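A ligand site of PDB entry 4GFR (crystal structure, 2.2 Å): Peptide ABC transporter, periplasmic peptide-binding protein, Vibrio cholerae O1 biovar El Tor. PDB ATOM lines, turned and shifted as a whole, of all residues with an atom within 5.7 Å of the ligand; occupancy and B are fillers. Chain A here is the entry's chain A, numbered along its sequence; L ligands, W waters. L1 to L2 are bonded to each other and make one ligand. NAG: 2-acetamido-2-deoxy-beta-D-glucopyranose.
An oxygen (O7) of NAG L1 lies within hydrogen-bond range of the guanidinium group (NH2) of Arg 435 (2.7 Å).
O7 of NAG L2 is in hydrogen-bond range of NE1 of Trp 512, at 2.9 Å.
OD1 of Asp 9 is in hydrogen-bond range of O6 of NAG L1 (2.6 Å).
ND2 of Asn 203 lies within hydrogen-bond range of O3 of NAG L2 (2.4 Å).
An oxygen (O4) of NAG L2 is in hydrogen-bond range of the side-chain carboxylate (OD1) of Asp 364, at 2.6 Å.
O3 of NAG L2 is in hydrogen-bond range of N of Phe 221 (3.2 Å).
An oxygen (O7) of NAG L2 lies close to the backbone NH (N) of Ser 220 (3.2 Å).
The side-chain amide nitrogen (ND2) of Asn 408 is in hydrogen-bond range of an oxygen (O3) of NAG L1.
N of Asn 203 sits close to O of Gly 361.
The backbone carbonyl oxygen (O) of Ser 219 is in hydrogen-bond range of the indole nitrogen (NE1) of Trp 512 (3.0 Å).
NE of Arg 435 is in hydrogen-bond range of OG1 of Thr 407 (2.8 Å).
O of Met 488 lies close to OG of Ser 219, at 3.4 Å.
NH2 of Arg 435 sits at hydrogen-bond distance from OD1 of Asn 408 (3.0 Å).
The side-chain hydroxyl (OG1) of Thr 363 is in hydrogen-bond range of the side-chain amide oxygen (OD1) of Asn 203 (3.1 Å).
O7 of NAG L2 sits close to O of Ser 219 (2.8 Å).
Residues that only touch the ligand: Val 7 (3.5 Å), Pro 8 (3.5 Å), Phe 10 (3.6 Å), Trp 362 (3.6 Å), Phe 365 (3.6 Å), Tyr 409 (3.4 Å), Phe 410 (3.8 Å), Phe 436 (3.6 Å) and Met 488 (3.2 Å).
Hydrophobic or aromatic side chains that line the ligand: Phe 10, Phe 221, Trp 362, Phe 365, Phe 410, Phe 436, Met 488 and Trp 512.
Of the 26 residues printed, 18 come within 4 Å of the ligand.
The nearest printed residue that does not touch the ligand is Thr 363 (4.3 Å).
Water W6 lies within hydrogen-bond range of O6 of NAG L1 (2.6 Å), OD1 of Asp 9 (3.1 Å) and NE1 of Trp 362 (3.2 Å).
Water W4 lies within hydrogen-bond range of O1 of NAG L1 (2.6 Å) and O of Ala 513 (2.7 Å).
Water W7 bridges an oxygen (O1) of NAG L1 (2.7 Å) and the guanidinium group of Arg 435 (2.9 Å).
Water W3 lies within hydrogen-bond range of the backbone carbonyl oxygen (O) of Val 7 (2.6 Å), an oxygen (O7) of NAG L2 (2.7 Å), the backbone NH (N) of Ser 219 (2.8 Å) and the backbone NH (N) of Ser 220 (3.2 Å).
Water W2 lies within hydrogen-bond range of an oxygen (O6) of NAG L2 (2.8 Å), the side-chain amide oxygen (OE1) of Gln 246 (3.2 Å) and the side-chain amide nitrogen (ND2) of Asn 408 (3.2 Å).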
ATOM      1  N   VAL A   7      22.912  21.171  26.379  1.00  0.00           N
ATOM      2  CA  VAL A   7      22.544  19.976  27.124  1.00  0.00           C
ATOM      3  C   VAL A   7      22.460  18.748  26.217  1.00  0.00           C
ATOM      4  O   VAL A   7      21.368  18.300  25.850  1.00  0.00           O
ATOM      5  CB  VAL A   7      21.175  20.167  27.848  1.00  0.00           C
ATOM      6  CG1 VAL A   7      20.916  18.988  28.775  1.00  0.00           C
ATOM      7  CG2 VAL A   7      21.167  21.483  28.619  1.00  0.00           C
ATOM      8  N   PRO A   8      23.616  18.189  25.841  1.00  0.00           N
ATOM      9  CA  PRO A   8      23.592  17.006  24.976  1.00  0.00           C
ATOM     10  C   PRO A   8      23.149  15.744  25.721  1.00  0.00           C
ATOM     11  O   PRO A   8      22.774  14.761  25.093  1.00  0.00           O
ATOM     12  CB  PRO A   8      25.039  16.918  24.472  1.00  0.00           C
ATOM     13  CG  PRO A   8      25.824  17.531  25.586  1.00  0.00           C
ATOM     14  CD  PRO A   8      24.982  18.716  25.979  1.00  0.00           C
ATOM     15  N   ASP A   9      23.177  15.796  27.056  1.00  0.00           N
ATOM     16  CA  ASP A   9      22.747  14.651  27.851  1.00  0.00           C
ATOM     17  C   ASP A   9      22.570  14.975  29.351  1.00  0.00           C
ATOM     18  O   ASP A   9      23.146  15.943  29.869  1.00  0.00           O
ATOM     19  CB  ASP A   9      23.743  13.500  27.676  1.00  0.00           C
ATOM     20  CG  ASP A   9      23.185  12.163  28.147  1.00  0.00           C
ATOM     21  OD1 ASP A   9      21.952  12.040  28.261  1.00  0.00           O
ATOM     22  OD2 ASP A   9      23.981  11.231  28.378  1.00  0.00           O
ATOM     23  N   PHE A  10      21.778  14.160  30.030  1.00  0.00           N
ATOM     24  CA  PHE A  10      21.520  14.331  31.452  1.00  0.00           C
ATOM     25  C   PHE A  10      22.504  13.502  32.268  1.00  0.00           C
ATOM     26  O   PHE A  10      23.079  12.534  31.765  1.00  0.00           O
ATOM     27  CB  PHE A  10      20.094  13.876  31.789  1.00  0.00           C
ATOM     28  CG  PHE A  10      19.021  14.652  31.062  1.00  0.00           C
ATOM     29  CD1 PHE A  10      17.868  14.015  30.638  1.00  0.00           C
ATOM     30  CD2 PHE A  10      19.153  16.023  30.855  1.00  0.00           C
ATOM     31  CE1 PHE A  10      16.857  14.716  30.006  1.00  0.00           C
ATOM     32  CE2 PHE A  10      18.131  16.749  30.229  1.00  0.00           C
ATOM     33  CZ  PHE A  10      16.984  16.091  29.807  1.00  0.00           C
ATOM     34  N   ASN A 203      14.086  15.175  32.406  1.00  0.00           N
ATOM     35  CA  ASN A 203      13.212  16.081  31.675  1.00  0.00           C
ATOM     36  C   ASN A 203      12.497  17.083  32.580  1.00  0.00           C
ATOM     37  O   ASN A 203      12.188  18.186  32.132  1.00  0.00           O
ATOM     38  CB  ASN A 203      12.186  15.293  30.863  1.00  0.00           C
ATOM     39  CG  ASN A 203      12.765  14.735  29.574  1.00  0.00           C
ATOM     40  OD1 ASN A 203      12.079  14.041  28.821  1.00  0.00           O
ATOM     41  ND2 ASN A 203      14.019  15.065  29.296  1.00  0.00           N
ATOM     42  N   THR A 218      19.398  22.846  23.048  1.00  0.00           N
ATOM     43  CA  THR A 218      18.902  21.615  23.636  1.00  0.00           C
ATOM     44  C   THR A 218      18.156  20.748  22.619  1.00  0.00           C
ATOM     45  O   THR A 218      17.769  21.227  21.548  1.00  0.00           O
ATOM     46  CB  THR A 218      17.975  21.924  24.828  1.00  0.00           C
ATOM     47  OG1 THR A 218      16.916  22.791  24.403  1.00  0.00           O
ATOM     48  CG2 THR A 218      18.772  22.626  25.941  1.00  0.00           C
ATOM     49  N   SER A 219      17.991  19.476  22.948  1.00  0.00           N
ATOM     50  CA  SER A 219      17.301  18.548  22.054  1.00  0.00           C
ATOM     51  C   SER A 219      16.518  17.557  22.914  1.00  0.00           C
ATOM     52  O   SER A 219      16.483  16.364  22.627  1.00  0.00           O
ATOM     53  CB  SER A 219      18.313  17.789  21.189  1.00  0.00           C
ATOM     54  OG  SER A 219      19.122  18.681  20.441  1.00  0.00           O
ATOM     55  N   SER A 220      15.885  18.064  23.956  1.00  0.00           N
ATOM     56  CA  SER A 220      15.129  17.206  24.854  1.00  0.00           C
ATOM     57  C   SER A 220      13.639  17.198  24.537  1.00  0.00           C
ATOM     58  O   SER A 220      13.164  17.977  23.706  1.00  0.00           O
ATOM     59  CB  SER A 220      15.303  17.693  26.288  1.00  0.00           C
ATOM     60  OG  SER A 220      14.226  18.540  26.614  1.00  0.00           O
ATOM     61  N   PHE A 221      12.913  16.313  25.192  1.00  0.00           N
ATOM     62  CA  PHE A 221      11.469  16.262  25.008  1.00  0.00           C
ATOM     63  C   PHE A 221      10.921  17.392  25.863  1.00  0.00           C
ATOM     64  O   PHE A 221      11.340  17.574  27.007  1.00  0.00           O
ATOM     65  CB  PHE A 221      10.884  14.928  25.486  1.00  0.00           C
ATOM     66  CG  PHE A 221       9.408  14.972  25.757  1.00  0.00           C
ATOM     67  CD1 PHE A 221       8.926  15.111  27.048  1.00  0.00           C
ATOM     68  CD2 PHE A 221       8.493  14.914  24.703  1.00  0.00           C
ATOM     69  CE1 PHE A 221       7.558  15.205  27.311  1.00  0.00           C
ATOM     70  CE2 PHE A 221       7.121  15.011  24.949  1.00  0.00           C
ATOM     71  CZ  PHE A 221       6.651  15.158  26.257  1.00  0.00           C
ATOM     72  N   GLN A 246      10.717   4.476  16.246  1.00  0.00           N
ATOM     73  CA  GLN A 246      10.698   4.250  17.675  1.00  0.00           C
ATOM     74  C   GLN A 246       9.870   2.987  17.807  1.00  0.00           C
ATOM     75  O   GLN A 246       8.879   2.822  17.104  1.00  0.00           O
ATOM     76  CB  GLN A 246      10.036   5.416  18.421  1.00  0.00           C
ATOM     77  CG  GLN A 246      10.817   6.735  18.306  1.00  0.00           C
ATOM     78  CD  GLN A 246      10.322   7.808  19.266  1.00  0.00           C
ATOM     79  OE1 GLN A 246      10.788   8.944  19.225  1.00  0.00           O
ATOM     80  NE2 GLN A 246       9.379   7.457  20.133  1.00  0.00           N
ATOM     81  N   PHE A 286       3.546  12.196  23.247  1.00  0.00           N
ATOM     82  CA  PHE A 286       4.355  13.123  22.480  1.00  0.00           C
ATOM     83  C   PHE A 286       3.667  14.410  22.088  1.00  0.00           C
ATOM     84  O   PHE A 286       4.223  15.203  21.317  1.00  0.00           O
ATOM     85  CB  PHE A 286       4.903  12.419  21.235  1.00  0.00           C
ATOM     86  CG  PHE A 286       5.743  11.209  21.542  1.00  0.00           C
ATOM     87  CD1 PHE A 286       5.148   9.981  21.811  1.00  0.00           C
ATOM     88  CD2 PHE A 286       7.130  11.331  21.623  1.00  0.00           C
ATOM     89  CE1 PHE A 286       5.935   8.867  22.148  1.00  0.00           C
ATOM     90  CE2 PHE A 286       7.917  10.227  21.955  1.00  0.00           C
ATOM     91  CZ  PHE A 286       7.326   8.994  22.216  1.00  0.00           C
ATOM     92  N   GLY A 361      13.923   9.432  33.485  1.00  0.00           N
ATOM     93  CA  GLY A 361      14.100  10.819  33.075  1.00  0.00           C
ATOM     94  C   GLY A 361      13.558  11.119  31.681  1.00  0.00           C
ATOM     95  O   GLY A 361      13.221  12.265  31.376  1.00  0.00           O
ATOM     96  N   TRP A 362      13.508  10.101  30.828  1.00  0.00           N
ATOM     97  CA  TRP A 362      12.995  10.252  29.455  1.00  0.00           C
ATOM     98  C   TRP A 362      11.481  10.107  29.539  1.00  0.00           C
ATOM     99  O   TRP A 362      10.904   9.140  29.045  1.00  0.00           O
ATOM    100  CB  TRP A 362      13.563   9.149  28.546  1.00  0.00           C
ATOM    101  CG  TRP A 362      15.074   9.115  28.424  1.00  0.00           C
ATOM    102  CD1 TRP A 362      15.978   9.586  29.339  1.00  0.00           C
ATOM    103  CD2 TRP A 362      15.845   8.508  27.369  1.00  0.00           C
ATOM    104  NE1 TRP A 362      17.257   9.317  28.914  1.00  0.00           N
ATOM    105  CE2 TRP A 362      17.205   8.655  27.709  1.00  0.00           C
ATOM    106  CE3 TRP A 362      15.505   7.858  26.176  1.00  0.00           C
ATOM    107  CZ2 TRP A 362      18.239   8.177  26.904  1.00  0.00           C
ATOM    108  CZ3 TRP A 362      16.544   7.376  25.364  1.00  0.00           C
ATOM    109  CH2 TRP A 362      17.898   7.537  25.731  1.00  0.00           C
ATOM    110  N   THR A 363      10.843  11.089  30.176  1.00  0.00           N
ATOM    111  CA  THR A 363       9.394  11.093  30.395  1.00  0.00           C
ATOM    112  C   THR A 363       8.506  10.769  29.200  1.00  0.00           C
ATOM    113  O   THR A 363       7.453  10.153  29.372  1.00  0.00           O
ATOM    114  CB  THR A 363       8.951  12.444  30.962  1.00  0.00           C
ATOM    115  OG1 THR A 363       9.310  13.490  30.042  1.00  0.00           O
ATOM    116  CG2 THR A 363       9.624  12.707  32.310  1.00  0.00           C
ATOM    117  N   ASP A 364       8.895  11.192  28.005  1.00  0.00           N
ATOM    118  CA  ASP A 364       8.081  10.881  26.839  1.00  0.00           C
ATOM    119  C   ASP A 364       8.052   9.376  26.607  1.00  0.00           C
ATOM    120  O   ASP A 364       7.025   8.813  26.240  1.00  0.00           O
ATOM    121  CB  ASP A 364       8.588  11.643  25.603  1.00  0.00           C
ATOM    122  CG  ASP A 364      10.063  11.392  25.326  1.00  0.00           C
ATOM    123  OD1 ASP A 364      10.814  11.073  26.263  1.00  0.00           O
ATOM    124  OD2 ASP A 364      10.460  11.557  24.156  1.00  0.00           O
ATOM    125  N   PHE A 365       9.187   8.717  26.851  1.00  0.00           N
ATOM    126  CA  PHE A 365       9.278   7.264  26.697  1.00  0.00           C
ATOM    127  C   PHE A 365       8.603   6.589  27.878  1.00  0.00           C
ATOM    128  O   PHE A 365       7.870   5.615  27.706  1.00  0.00           O
ATOM    129  CB  PHE A 365      10.739   6.801  26.617  1.00  0.00           C
ATOM    130  CG  PHE A 365      11.376   6.998  25.260  1.00  0.00           C
ATOM    131  CD1 PHE A 365      12.567   6.350  24.929  1.00  0.00           C
ATOM    132  CD2 PHE A 365      10.778   7.827  24.307  1.00  0.00           C
ATOM    133  CE1 PHE A 365      13.140   6.518  23.664  1.00  0.00           C
ATOM    134  CE2 PHE A 365      11.347   7.999  23.050  1.00  0.00           C
ATOM    135  CZ  PHE A 365      12.532   7.346  22.731  1.00  0.00           C
ATOM    136  N   THR A 407      12.485   2.115  22.581  1.00  0.00           N
ATOM    137  CA  THR A 407      13.653   2.882  22.206  1.00  0.00           C
ATOM    138  C   THR A 407      13.469   3.539  20.857  1.00  0.00           C
ATOM    139  O   THR A 407      12.556   3.213  20.109  1.00  0.00           O
ATOM    140  CB  THR A 407      14.913   1.983  22.109  1.00  0.00           C
ATOM    141  OG1 THR A 407      16.064   2.800  21.828  1.00  0.00           O
ATOM    142  CG2 THR A 407      14.755   0.955  20.979  1.00  0.00           C
ATOM    143  N   ASN A 408      14.350   4.479  20.566  1.00  0.00           N
ATOM    144  CA  ASN A 408      14.355   5.150  19.270  1.00  0.00           C
ATOM    145  C   ASN A 408      15.619   4.619  18.607  1.00  0.00           C
ATOM    146  O   ASN A 408      16.339   3.815  19.206  1.00  0.00           O
ATOM    147  CB  ASN A 408      14.424   6.667  19.442  1.00  0.00           C
ATOM    148  CG  ASN A 408      15.518   7.105  20.409  1.00  0.00           C
ATOM    149  OD1 ASN A 408      16.163   6.289  21.045  1.00  0.00           O
ATOM    150  ND2 ASN A 408      15.706   8.419  20.521  1.00  0.00           N
ATOM    151  N   TYR A 409      15.885   5.049  17.378  1.00  0.00           N
ATOM    152  CA  TYR A 409      17.075   4.611  16.655  1.00  0.00           C
ATOM    153  C   TYR A 409      17.667   5.809  15.966  1.00  0.00           C
ATOM    154  O   TYR A 409      17.053   6.871  15.943  1.00  0.00           O
ATOM    155  CB  TYR A 409      16.708   3.596  15.563  1.00  0.00           C
ATOM    156  CG  TYR A 409      16.108   2.301  16.049  1.00  0.00           C
ATOM    157  CD1 TYR A 409      16.900   1.155  16.196  1.00  0.00           C
ATOM    158  CD2 TYR A 409      14.747   2.201  16.330  1.00  0.00           C
ATOM    159  CE1 TYR A 409      16.351  -0.046  16.626  1.00  0.00           C
ATOM    160  CE2 TYR A 409      14.190   1.007  16.750  1.00  0.00           C
ATOM    161  CZ  TYR A 409      14.990  -0.120  16.893  1.00  0.00           C
ATOM    162  OH  TYR A 409      14.435  -1.288  17.341  1.00  0.00           O
ATOM    163  N   PHE A 410      18.859   5.661  15.404  1.00  0.00           N
ATOM    164  CA  PHE A 410      19.457   6.764  14.664  1.00  0.00           C
ATOM    165  C   PHE A 410      18.781   6.728  13.296  1.00  0.00           C
ATOM    166  O   PHE A 410      18.183   5.727  12.926  1.00  0.00           O
ATOM    167  CB  PHE A 410      20.974   6.636  14.598  1.00  0.00           C
ATOM    168  CG  PHE A 410      21.660   7.256  15.787  1.00  0.00           C
ATOM    169  CD1 PHE A 410      21.878   8.626  15.836  1.00  0.00           C
ATOM    170  CD2 PHE A 410      21.986   6.482  16.899  1.00  0.00           C
ATOM    171  CE1 PHE A 410      22.406   9.226  16.983  1.00  0.00           C
ATOM    172  CE2 PHE A 410      22.505   7.071  18.046  1.00  0.00           C
ATOM    173  CZ  PHE A 410      22.715   8.448  18.086  1.00  0.00           C
ATOM    174  N   ARG A 435      22.772  -0.339  21.990  1.00  0.00           N
ATOM    175  CA  ARG A 435      21.645  -1.238  22.266  1.00  0.00           C
ATOM    176  C   ARG A 435      20.795  -1.656  21.069  1.00  0.00           C
ATOM    177  O   ARG A 435      20.196  -2.724  21.064  1.00  0.00           O
ATOM    178  CB  ARG A 435      20.714  -0.550  23.277  1.00  0.00           C
ATOM    179  CG  ARG A 435      20.100   0.748  22.717  1.00  0.00           C
ATOM    180  CD  ARG A 435      19.203   1.454  23.741  1.00  0.00           C
ATOM    181  NE  ARG A 435      18.501   2.614  23.197  1.00  0.00           N
ATOM    182  CZ  ARG A 435      19.076   3.778  22.911  1.00  0.00           C
ATOM    183  NH1 ARG A 435      20.383   3.937  23.103  1.00  0.00           N
ATOM    184  NH2 ARG A 435      18.344   4.792  22.453  1.00  0.00           N
ATOM    185  N   PHE A 436      20.738  -0.796  20.064  1.00  0.00           N
ATOM    186  CA  PHE A 436      19.905  -0.994  18.877  1.00  0.00           C
ATOM    187  C   PHE A 436      19.636  -2.385  18.252  1.00  0.00           C
ATOM    188  O   PHE A 436      18.510  -2.673  17.868  1.00  0.00           O
ATOM    189  CB  PHE A 436      20.361  -0.009  17.803  1.00  0.00           C
ATOM    190  CG  PHE A 436      20.454   1.404  18.313  1.00  0.00           C
ATOM    191  CD1 PHE A 436      19.330   2.030  18.859  1.00  0.00           C
ATOM    192  CD2 PHE A 436      21.668   2.076  18.336  1.00  0.00           C
ATOM    193  CE1 PHE A 436      19.423   3.317  19.410  1.00  0.00           C
ATOM    194  CE2 PHE A 436      21.766   3.359  18.879  1.00  0.00           C
ATOM    195  CZ  PHE A 436      20.639   3.970  19.419  1.00  0.00           C
ATOM    196  N   TRP A 487      13.723  14.969  15.372  1.00  0.00           N
ATOM    197  CA  TRP A 487      14.917  15.450  16.039  1.00  0.00           C
ATOM    198  C   TRP A 487      14.548  16.630  16.947  1.00  0.00           C
ATOM    199  O   TRP A 487      14.727  17.789  16.557  1.00  0.00           O
ATOM    200  CB  TRP A 487      15.957  15.920  15.015  1.00  0.00           C
ATOM    201  CG  TRP A 487      16.437  14.859  14.077  1.00  0.00           C
ATOM    202  CD1 TRP A 487      16.209  14.795  12.733  1.00  0.00           C
ATOM    203  CD2 TRP A 487      17.239  13.716  14.401  1.00  0.00           C
ATOM    204  NE1 TRP A 487      16.816  13.685  12.197  1.00  0.00           N
ATOM    205  CE2 TRP A 487      17.453  13.007  13.200  1.00  0.00           C
ATOM    206  CE3 TRP A 487      17.789  13.218  15.591  1.00  0.00           C
ATOM    207  CZ2 TRP A 487      18.203  11.817  13.159  1.00  0.00           C
ATOM    208  CZ3 TRP A 487      18.526  12.039  15.548  1.00  0.00           C
ATOM    209  CH2 TRP A 487      18.726  11.358  14.336  1.00  0.00           C
ATOM    210  N   MET A 488      14.036  16.340  18.134  1.00  0.00           N
ATOM    211  CA  MET A 488      13.681  17.427  19.062  1.00  0.00           C
ATOM    212  C   MET A 488      14.856  18.383  19.129  1.00  0.00           C
ATOM    213  O   MET A 488      16.010  17.959  19.219  1.00  0.00           O
ATOM    214  CB  MET A 488      13.388  16.886  20.465  1.00  0.00           C
ATOM    215  CG  MET A 488      12.273  15.858  20.542  1.00  0.00           C
ATOM    216  SD  MET A 488      12.972  14.196  20.525  1.00  0.00           S
ATOM    217  CE  MET A 488      13.826  14.193  22.124  1.00  0.00           C
ATOM    218  N   TRP A 512      22.823  16.266  20.381  1.00  0.00           N
ATOM    219  CA  TRP A 512      23.179  14.984  20.984  1.00  0.00           C
ATOM    220  C   TRP A 512      24.498  14.474  20.426  1.00  0.00           C
ATOM    221  O   TRP A 512      24.821  14.715  19.271  1.00  0.00           O
ATOM    222  CB  TRP A 512      22.120  13.897  20.695  1.00  0.00           C
ATOM    223  CG  TRP A 512      20.724  14.125  21.210  1.00  0.00           C
ATOM    224  CD1 TRP A 512      20.359  14.827  22.327  1.00  0.00           C
ATOM    225  CD2 TRP A 512      19.514  13.578  20.673  1.00  0.00           C
ATOM    226  NE1 TRP A 512      19.003  14.748  22.520  1.00  0.00           N
ATOM    227  CE2 TRP A 512      18.456  13.994  21.509  1.00  0.00           C
ATOM    228  CE3 TRP A 512      19.216  12.787  19.559  1.00  0.00           C
ATOM    229  CZ2 TRP A 512      17.128  13.625  21.285  1.00  0.00           C
ATOM    230  CZ3 TRP A 512      17.894  12.414  19.327  1.00  0.00           C
ATOM    231  CH2 TRP A 512      16.865  12.843  20.189  1.00  0.00           C
ATOM    232  N   ALA A 513      25.259  13.758  21.256  1.00  0.00           N
ATOM    233  CA  ALA A 513      26.498  13.159  20.785  1.00  0.00           C
ATOM    234  C   ALA A 513      25.960  12.136  19.780  1.00  0.00           C
ATOM    235  O   ALA A 513      24.859  11.613  19.976  1.00  0.00           O
ATOM    236  CB  ALA A 513      27.215  12.446  21.939  1.00  0.00           C
HETATM  237  C1  NAG L   1      20.810   9.835  22.260  1.00  0.00           C
HETATM  238  C2  NAG L   1      19.327   9.401  22.100  1.00  0.00           C
HETATM  239  C3  NAG L   1      18.355  10.501  22.584  1.00  0.00           C
HETATM  240  C4  NAG L   1      18.733  11.016  23.993  1.00  0.00           C
HETATM  241  C5  NAG L   1      20.217  11.430  24.007  1.00  0.00           C
HETATM  242  C6  NAG L   1      20.695  11.937  25.383  1.00  0.00           C
HETATM  243  C7  NAG L   1      19.069   7.856  20.248  1.00  0.00           C
HETATM  244  C8  NAG L   1      18.790   7.658  18.758  1.00  0.00           C
HETATM  245  N2  NAG L   1      19.061   9.113  20.695  1.00  0.00           N
HETATM  246  O1  NAG L   1      21.644   8.757  22.004  1.00  0.00           O
HETATM  247  O3  NAG L   1      17.041   9.954  22.623  1.00  0.00           O
HETATM  248  O4  NAG L   1      17.953  12.179  24.346  1.00  0.00           O
HETATM  249  O5  NAG L   1      21.052  10.286  23.628  1.00  0.00           O
HETATM  250  O6  NAG L   1      20.549  10.931  26.385  1.00  0.00           O
HETATM  251  O7  NAG L   1      19.304   6.869  20.978  1.00  0.00           O
HETATM  252  C1  NAG L   2      16.869  12.057  25.192  1.00  0.00           C
HETATM  253  C2  NAG L   2      16.460  13.443  25.698  1.00  0.00           C
HETATM  254  C3  NAG L   2      15.238  13.286  26.603  1.00  0.00           C
HETATM  255  C4  NAG L   2      14.093  12.647  25.790  1.00  0.00           C
HETATM  256  C5  NAG L   2      14.578  11.237  25.282  1.00  0.00           C
HETATM  257  C6  NAG L   2      13.563  10.495  24.428  1.00  0.00           C
HETATM  258  C7  NAG L   2      18.177  15.164  26.029  1.00  0.00           C
HETATM  259  C8  NAG L   2      19.317  15.673  26.895  1.00  0.00           C
HETATM  260  N2  NAG L   2      17.570  14.036  26.446  1.00  0.00           N
HETATM  261  O3  NAG L   2      14.834  14.568  27.063  1.00  0.00           O
HETATM  262  O4  NAG L   2      12.924  12.502  26.632  1.00  0.00           O
HETATM  263  O5  NAG L   2      15.777  11.396  24.466  1.00  0.00           O
HETATM  264  O6  NAG L   2      13.049  11.301  23.371  1.00  0.00           O
HETATM  265  O7  NAG L   2      17.857  15.781  25.006  1.00  0.00           O
HETATM  266  O   HOH W   1      24.107  10.372  24.590  1.00  0.00           O
HETATM  267  O   HOH W   2      13.188  10.377  20.761  1.00  0.00           O
HETATM  268  O   HOH W   3      18.767  18.348  25.369  1.00  0.00           O
HETATM  269  O   HOH W   4      24.066   9.501  21.370  1.00  0.00           O
HETATM  270  O   HOH W   5      21.967   8.265  25.545  1.00  0.00           O
HETATM  271  O   HOH W   6      18.839  12.001  28.026  1.00  0.00           O
HETATM  272  O   HOH W   7      21.644   6.517  23.587  1.00  0.00           O
